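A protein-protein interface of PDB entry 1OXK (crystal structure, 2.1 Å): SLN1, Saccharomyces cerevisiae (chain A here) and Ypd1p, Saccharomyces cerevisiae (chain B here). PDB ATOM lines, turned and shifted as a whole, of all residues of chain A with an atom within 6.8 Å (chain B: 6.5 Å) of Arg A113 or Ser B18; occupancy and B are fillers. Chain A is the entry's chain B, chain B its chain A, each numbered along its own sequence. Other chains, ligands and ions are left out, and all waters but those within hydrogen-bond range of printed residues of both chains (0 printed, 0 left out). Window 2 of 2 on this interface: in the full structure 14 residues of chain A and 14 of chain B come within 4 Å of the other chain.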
ATOM      1  N   ARG A  19      31.637 -12.800 -31.628  1.00  0.00           N
ATOM      2  CA  ARG A  19      31.551 -11.594 -30.844  1.00  0.00           C
ATOM      3  C   ARG A  19      31.796 -11.931 -29.371  1.00  0.00           C
ATOM      4  O   ARG A  19      32.565 -11.239 -28.705  1.00  0.00           O
ATOM      5  CB  ARG A  19      30.175 -10.939 -31.008  1.00  0.00           C
ATOM      6  CG  ARG A  19      30.003  -9.594 -30.272  1.00  0.00           C
ATOM      7  CD  ARG A  19      30.945  -8.517 -30.737  1.00  0.00           C
ATOM      8  NE  ARG A  19      30.647  -7.278 -30.035  1.00  0.00           N
ATOM      9  CZ  ARG A  19      31.392  -6.188 -30.076  1.00  0.00           C
ATOM     10  NH1 ARG A  19      31.013  -5.118 -29.382  1.00  0.00           N
ATOM     11  NH2 ARG A  19      32.495  -6.146 -30.821  1.00  0.00           N
ATOM     12  N   MET A  20      31.144 -12.970 -28.853  1.00  0.00           N
ATOM     13  CA  MET A  20      31.355 -13.356 -27.467  1.00  0.00           C
ATOM     14  C   MET A  20      32.844 -13.627 -27.210  1.00  0.00           C
ATOM     15  O   MET A  20      33.424 -13.159 -26.234  1.00  0.00           O
ATOM     16  CB  MET A  20      30.546 -14.608 -27.098  1.00  0.00           C
ATOM     17  CG  MET A  20      29.183 -14.330 -26.565  1.00  0.00           C
ATOM     18  SD  MET A  20      28.136 -15.764 -26.338  1.00  0.00           S
ATOM     19  CE  MET A  20      26.590 -15.017 -26.527  1.00  0.00           C
ATOM     20  N   LEU A  21      33.479 -14.371 -28.094  1.00  0.00           N
ATOM     21  CA  LEU A  21      34.881 -14.678 -27.892  1.00  0.00           C
ATOM     22  C   LEU A  21      35.756 -13.408 -27.970  1.00  0.00           C
ATOM     23  O   LEU A  21      36.677 -13.248 -27.167  1.00  0.00           O
ATOM     24  CB  LEU A  21      35.341 -15.722 -28.903  1.00  0.00           C
ATOM     25  CG  LEU A  21      34.619 -17.074 -28.708  1.00  0.00           C
ATOM     26  CD1 LEU A  21      34.695 -17.889 -29.944  1.00  0.00           C
ATOM     27  CD2 LEU A  21      35.173 -17.825 -27.551  1.00  0.00           C
ATOM     28  N   LEU A  23      34.904 -10.389 -27.193  1.00  0.00           N
ATOM     29  CA  LEU A  23      34.722  -9.655 -25.945  1.00  0.00           C
ATOM     30  C   LEU A  23      35.460 -10.310 -24.771  1.00  0.00           C
ATOM     31  O   LEU A  23      35.642  -9.695 -23.713  1.00  0.00           O
ATOM     32  CB  LEU A  23      33.210  -9.511 -25.638  1.00  0.00           C
ATOM     33  CG  LEU A  23      32.518  -8.160 -25.954  1.00  0.00           C
ATOM     34  CD1 LEU A  23      33.348  -7.181 -26.793  1.00  0.00           C
ATOM     35  CD2 LEU A  23      31.159  -8.360 -26.591  1.00  0.00           C
ATOM     36  N   GLU A  24      35.879 -11.560 -24.932  1.00  0.00           N
ATOM     37  CA  GLU A  24      36.581 -12.256 -23.876  1.00  0.00           C
ATOM     38  C   GLU A  24      38.062 -12.208 -24.170  1.00  0.00           C
ATOM     39  O   GLU A  24      38.856 -12.914 -23.551  1.00  0.00           O
ATOM     40  CB  GLU A  24      36.137 -13.716 -23.763  1.00  0.00           C
ATOM     41  CG  GLU A  24      34.765 -13.904 -23.151  1.00  0.00           C
ATOM     42  CD  GLU A  24      34.689 -13.378 -21.722  1.00  0.00           C
ATOM     43  OE1 GLU A  24      35.759 -13.270 -21.096  1.00  0.00           O
ATOM     44  OE2 GLU A  24      33.585 -13.063 -21.204  1.00  0.00           O
ATOM     45  N   LEU A 107      27.336 -26.115 -24.134  1.00  0.00           N
ATOM     46  CA  LEU A 107      26.712 -24.810 -23.972  1.00  0.00           C
ATOM     47  C   LEU A 107      25.351 -24.945 -24.612  1.00  0.00           C
ATOM     48  O   LEU A 107      25.247 -25.423 -25.730  1.00  0.00           O
ATOM     49  CB  LEU A 107      27.463 -23.731 -24.721  1.00  0.00           C
ATOM     50  CG  LEU A 107      28.777 -23.251 -24.131  1.00  0.00           C
ATOM     51  CD1 LEU A 107      29.485 -22.398 -25.124  1.00  0.00           C
ATOM     52  CD2 LEU A 107      28.544 -22.480 -22.816  1.00  0.00           C
ATOM     53  N   PRO A 110      19.884 -20.663 -26.557  1.00  0.00           N
ATOM     54  CA  PRO A 110      20.772 -19.607 -27.029  1.00  0.00           C
ATOM     55  C   PRO A 110      21.932 -19.456 -26.104  1.00  0.00           C
ATOM     56  O   PRO A 110      21.741 -19.471 -24.889  1.00  0.00           O
ATOM     57  CB  PRO A 110      19.899 -18.351 -26.936  1.00  0.00           C
ATOM     58  CG  PRO A 110      18.901 -18.639 -25.862  1.00  0.00           C
ATOM     59  CD  PRO A 110      18.666 -20.116 -25.924  1.00  0.00           C
ATOM     60  N   ILE A 111      23.111 -19.290 -26.677  1.00  0.00           N
ATOM     61  CA  ILE A 111      24.331 -19.252 -25.912  1.00  0.00           C
ATOM     62  C   ILE A 111      24.274 -18.109 -24.933  1.00  0.00           C
ATOM     63  O   ILE A 111      23.896 -16.999 -25.267  1.00  0.00           O
ATOM     64  CB  ILE A 111      25.554 -19.116 -26.849  1.00  0.00           C
ATOM     65  CG1 ILE A 111      25.517 -20.183 -27.935  1.00  0.00           C
ATOM     66  CG2 ILE A 111      26.847 -19.207 -26.074  1.00  0.00           C
ATOM     67  CD1 ILE A 111      25.237 -21.531 -27.430  1.00  0.00           C
ATOM     68  N   LYS A 112      24.591 -18.381 -23.695  1.00  0.00           N
ATOM     69  CA  LYS A 112      24.656 -17.310 -22.715  1.00  0.00           C
ATOM     70  C   LYS A 112      26.122 -16.996 -22.387  1.00  0.00           C
ATOM     71  O   LYS A 112      26.909 -17.884 -22.011  1.00  0.00           O
ATOM     72  CB  LYS A 112      23.924 -17.702 -21.522  1.00  0.00           C
ATOM     73  N   ARG A 113      26.478 -15.714 -22.482  1.00  0.00           N
ATOM     74  CA  ARG A 113      27.862 -15.294 -22.323  1.00  0.00           C
ATOM     75  C   ARG A 113      28.559 -15.788 -21.038  1.00  0.00           C
ATOM     76  O   ARG A 113      29.681 -16.256 -21.109  1.00  0.00           O
ATOM     77  CB  ARG A 113      27.978 -13.782 -22.478  1.00  0.00           C
ATOM     78  CG  ARG A 113      29.403 -13.324 -22.560  1.00  0.00           C
ATOM     79  CD  ARG A 113      29.635 -12.206 -23.547  1.00  0.00           C
ATOM     80  NE  ARG A 113      28.723 -11.096 -23.302  1.00  0.00           N
ATOM     81  CZ  ARG A 113      29.093  -9.869 -22.964  1.00  0.00           C
ATOM     82  NH1 ARG A 113      30.367  -9.544 -22.855  1.00  0.00           N
ATOM     83  NH2 ARG A 113      28.163  -8.942 -22.775  1.00  0.00           N
ATOM     84  N   PRO A 114      27.922 -15.680 -19.879  1.00  0.00           N
ATOM     85  CA  PRO A 114      28.543 -16.165 -18.640  1.00  0.00           C
ATOM     86  C   PRO A 114      28.890 -17.647 -18.710  1.00  0.00           C
ATOM     87  O   PRO A 114      29.898 -18.038 -18.200  1.00  0.00           O
ATOM     88  CB  PRO A 114      27.459 -15.935 -17.583  1.00  0.00           C
ATOM     89  CG  PRO A 114      26.535 -14.898 -18.214  1.00  0.00           C
ATOM     90  CD  PRO A 114      26.595 -15.099 -19.655  1.00  0.00           C
ATOM     91  N   LYS A 115      28.063 -18.447 -19.361  1.00  0.00           N
ATOM     92  CA  LYS A 115      28.368 -19.855 -19.517  1.00  0.00           C
ATOM     93  C   LYS A 115      29.556 -20.048 -20.430  1.00  0.00           C
ATOM     94  O   LYS A 115      30.428 -20.839 -20.169  1.00  0.00           O
ATOM     95  CB  LYS A 115      27.146 -20.564 -20.044  1.00  0.00           C
ATOM     96  CG  LYS A 115      25.950 -20.489 -19.072  1.00  0.00           C
ATOM     97  CD  LYS A 115      26.186 -21.336 -17.843  1.00  0.00           C
ATOM     98  CE  LYS A 115      24.898 -21.470 -17.001  1.00  0.00           C
ATOM     99  NZ  LYS A 115      25.086 -22.406 -15.827  1.00  0.00           N
ATOM    100  N   LEU A 116      29.634 -19.244 -21.477  1.00  0.00           N
ATOM    101  CA  LEU A 116      30.770 -19.278 -22.388  1.00  0.00           C
ATOM    102  C   LEU A 116      32.045 -18.911 -21.628  1.00  0.00           C
ATOM    103  O   LEU A 116      33.078 -19.589 -21.749  1.00  0.00           O
ATOM    104  CB  LEU A 116      30.536 -18.296 -23.542  1.00  0.00           C
ATOM    105  CG  LEU A 116      31.559 -18.278 -24.691  1.00  0.00           C
ATOM    106  CD1 LEU A 116      32.577 -17.233 -24.432  1.00  0.00           C
ATOM    107  CD2 LEU A 116      32.244 -19.597 -24.889  1.00  0.00           C
ATOM    108  N   LYS A 117      31.975 -17.865 -20.808  1.00  0.00           N
ATOM    109  CA  LYS A 117      33.134 -17.457 -20.004  1.00  0.00           C
ATOM    110  C   LYS A 117      33.625 -18.617 -19.112  1.00  0.00           C
ATOM    111  O   LYS A 117      34.811 -18.872 -19.016  1.00  0.00           O
ATOM    112  CB  LYS A 117      32.796 -16.240 -19.118  1.00  0.00           C
ATOM    113  N   THR A 118      32.709 -19.289 -18.439  1.00  0.00           N
ATOM    114  CA  THR A 118      33.068 -20.408 -17.568  1.00  0.00           C
ATOM    115  C   THR A 118      33.759 -21.558 -18.347  1.00  0.00           C
ATOM    116  O   THR A 118      34.770 -22.094 -17.896  1.00  0.00           O
ATOM    117  CB  THR A 118      31.798 -20.896 -16.891  1.00  0.00           C
ATOM    118  OG1 THR A 118      31.301 -19.871 -16.024  1.00  0.00           O
ATOM    119  CG2 THR A 118      32.066 -22.048 -15.966  1.00  0.00           C
ATOM    120  N   LEU B  13      17.147 -11.605 -26.982  1.00  0.00           N
ATOM    121  CA  LEU B  13      17.794 -10.512 -27.765  1.00  0.00           C
ATOM    122  C   LEU B  13      18.671  -9.627 -26.901  1.00  0.00           C
ATOM    123  O   LEU B  13      19.736  -9.189 -27.347  1.00  0.00           O
ATOM    124  CB  LEU B  13      16.762  -9.674 -28.502  1.00  0.00           C
ATOM    125  CG  LEU B  13      17.270  -8.644 -29.529  1.00  0.00           C
ATOM    126  CD1 LEU B  13      18.184  -9.280 -30.564  1.00  0.00           C
ATOM    127  CD2 LEU B  13      16.112  -8.047 -30.248  1.00  0.00           C
ATOM    128  N   ASN B  14      18.244  -9.403 -25.656  1.00  0.00           N
ATOM    129  CA  ASN B  14      19.029  -8.600 -24.715  1.00  0.00           C
ATOM    130  C   ASN B  14      20.450  -9.134 -24.541  1.00  0.00           C
ATOM    131  O   ASN B  14      21.369  -8.373 -24.356  1.00  0.00           O
ATOM    132  CB  ASN B  14      18.321  -8.413 -23.372  1.00  0.00           C
ATOM    133  CG  ASN B  14      17.243  -7.354 -23.459  1.00  0.00           C
ATOM    134  OD1 ASN B  14      17.204  -6.616 -24.434  1.00  0.00           O
ATOM    135  ND2 ASN B  14      16.325  -7.320 -22.488  1.00  0.00           N
ATOM    136  N   GLU B  15      20.646 -10.444 -24.645  1.00  0.00           N
ATOM    137  CA  GLU B  15      22.010 -10.999 -24.550  1.00  0.00           C
ATOM    138  C   GLU B  15      22.888 -10.490 -25.684  1.00  0.00           C
ATOM    139  O   GLU B  15      24.085 -10.203 -25.538  1.00  0.00           O
ATOM    140  CB  GLU B  15      22.025 -12.537 -24.638  1.00  0.00           C
ATOM    141  CG  GLU B  15      21.916 -13.255 -23.298  1.00  0.00           C
ATOM    142  CD  GLU B  15      23.130 -13.035 -22.416  1.00  0.00           C
ATOM    143  OE1 GLU B  15      24.159 -13.718 -22.676  1.00  0.00           O
ATOM    144  OE2 GLU B  15      23.050 -12.181 -21.470  1.00  0.00           O
ATOM    145  N   ILE B  16      22.301 -10.432 -26.854  1.00  0.00           N
ATOM    146  CA  ILE B  16      23.031  -9.976 -27.994  1.00  0.00           C
ATOM    147  C   ILE B  16      23.313  -8.492 -27.860  1.00  0.00           C
ATOM    148  O   ILE B  16      24.446  -8.081 -28.074  1.00  0.00           O
ATOM    149  CB  ILE B  16      22.247 -10.307 -29.255  1.00  0.00           C
ATOM    150  CG1 ILE B  16      22.265 -11.836 -29.439  1.00  0.00           C
ATOM    151  CG2 ILE B  16      22.896  -9.635 -30.440  1.00  0.00           C
ATOM    152  CD1 ILE B  16      21.344 -12.302 -30.474  1.00  0.00           C
ATOM    153  N   ILE B  17      22.310  -7.720 -27.430  1.00  0.00           N
ATOM    154  CA  ILE B  17      22.454  -6.277 -27.264  1.00  0.00           C
ATOM    155  C   ILE B  17      23.476  -5.946 -26.176  1.00  0.00           C
ATOM    156  O   ILE B  17      24.224  -4.991 -26.312  1.00  0.00           O
ATOM    157  CB  ILE B  17      21.102  -5.622 -27.003  1.00  0.00           C
ATOM    158  CG1 ILE B  17      20.239  -5.696 -28.277  1.00  0.00           C
ATOM    159  CG2 ILE B  17      21.295  -4.142 -26.586  1.00  0.00           C
ATOM    160  CD1 ILE B  17      18.763  -5.384 -28.051  1.00  0.00           C
ATOM    161  N   SER B  18      23.584  -6.757 -25.134  1.00  0.00           N
ATOM    162  CA  SER B  18      24.559  -6.490 -24.088  1.00  0.00           C
ATOM    163  C   SER B  18      25.945  -6.495 -24.664  1.00  0.00           C
ATOM    164  O   SER B  18      26.875  -6.071 -24.019  1.00  0.00           O
ATOM    165  CB  SER B  18      24.542  -7.554 -22.979  1.00  0.00           C
ATOM    166  OG  SER B  18      25.264  -8.759 -23.355  1.00  0.00           O
ATOM    167  N   MET B  19      26.101  -7.036 -25.865  1.00  0.00           N
ATOM    168  CA  MET B  19      27.404  -7.072 -26.461  1.00  0.00           C
ATOM    169  C   MET B  19      27.665  -5.896 -27.356  1.00  0.00           C
ATOM    170  O   MET B  19      28.705  -5.857 -27.990  1.00  0.00           O
ATOM    171  CB  MET B  19      27.581  -8.349 -27.255  1.00  0.00           C
ATOM    172  CG  MET B  19      27.610  -9.550 -26.376  1.00  0.00           C
ATOM    173  SD  MET B  19      28.018 -11.038 -27.290  1.00  0.00           S
ATOM    174  CE  MET B  19      29.114 -11.505 -26.298  1.00  0.00           C
ATOM    175  N   ASP B  20      26.743  -4.942 -27.413  1.00  0.00           N
ATOM    176  CA  ASP B  20      26.985  -3.729 -28.189  1.00  0.00           C
ATOM    177  C   ASP B  20      28.022  -2.861 -27.482  1.00  0.00           C
ATOM    178  O   ASP B  20      28.921  -2.311 -28.138  1.00  0.00           O
ATOM    179  CB  ASP B  20      25.690  -2.927 -28.401  1.00  0.00           C
ATOM    180  CG  ASP B  20      24.817  -3.510 -29.502  1.00  0.00           C
ATOM    181  OD1 ASP B  20      25.381  -3.991 -30.503  1.00  0.00           O
ATOM    182  OD2 ASP B  20      23.565  -3.519 -29.462  1.00  0.00           O
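O of Glu B15 sits at hydrogen-bond distance from OG of Ser B18 (2.9 Å).
Of the 8 printed residues of chain B, 4 touch a printed residue of chain A.
Printed residues of chain B that touch a printed residue of chain A: Glu B15, Ser B18, Met B19 and Asp B20.
Along chain B the printed residues that touch a printed residue of chain A span positions 15 to 20.
Among the printed residues, no Asp or Glu carboxylate lies within 4 Å of a Lys or Arg side-chain nitrogen of the other chain.
Of chain B, only Glu B15, Ser B18 and Met B19 come within 4 Å of Arg A113.
Ser B18 touches one residue of chain A.
Of the printed residues of chain B, Leu A23 touches Met B19 (3.6 Å).
Of the printed residues of chain A, Met B19 touches Arg A19, Met A20, Leu A23 and Arg A113.
Of the printed residues of chain B, Arg A19 touches Met B19 (2.8 Å) and Asp B20 (3.7 Å).
Of the printed residues of chain A, Asp B20 touches Arg A19 (3.7 Å).
Lys A117 touches none of the printed residues of chain B.
The nearest residue of chain B that does not touch Arg A113 is Asp B20 (6.3 Å).
The nearest residue of chain A that does not touch Ser B18 is Leu A23 (5.5 Å).
The nearest printed residue of chain A that does not touch Glu B15 is Pro A114 (4.1 Å).
Among the printed residues, pairs that only touch across the chains: Arg A19 with Asp B20 (3.7 Å), Met A20 with Met B19 (2.8 Å), Leu A23 with Met B19 (3.6 Å), Lys A112 with Glu B15 (3.6 Å) and Arg A113 with Met B19 (2.9 Å).
The backbone carbonyl oxygen (O) of Met B19 lies within hydrogen-bond range of the guanidinium group (NH1) of Arg A19 (2.8 Å).
The side-chain hydroxyl (OG) of Ser B18 is in hydrogen-bond range of the guanidinium group (NH2) of Arg A113 (3.0 Å).
The backbone NH (N) of Arg A113 sits at hydrogen-bond distance from the side-chain carboxylate (OE1) of Glu B15, 3.1 Å away.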
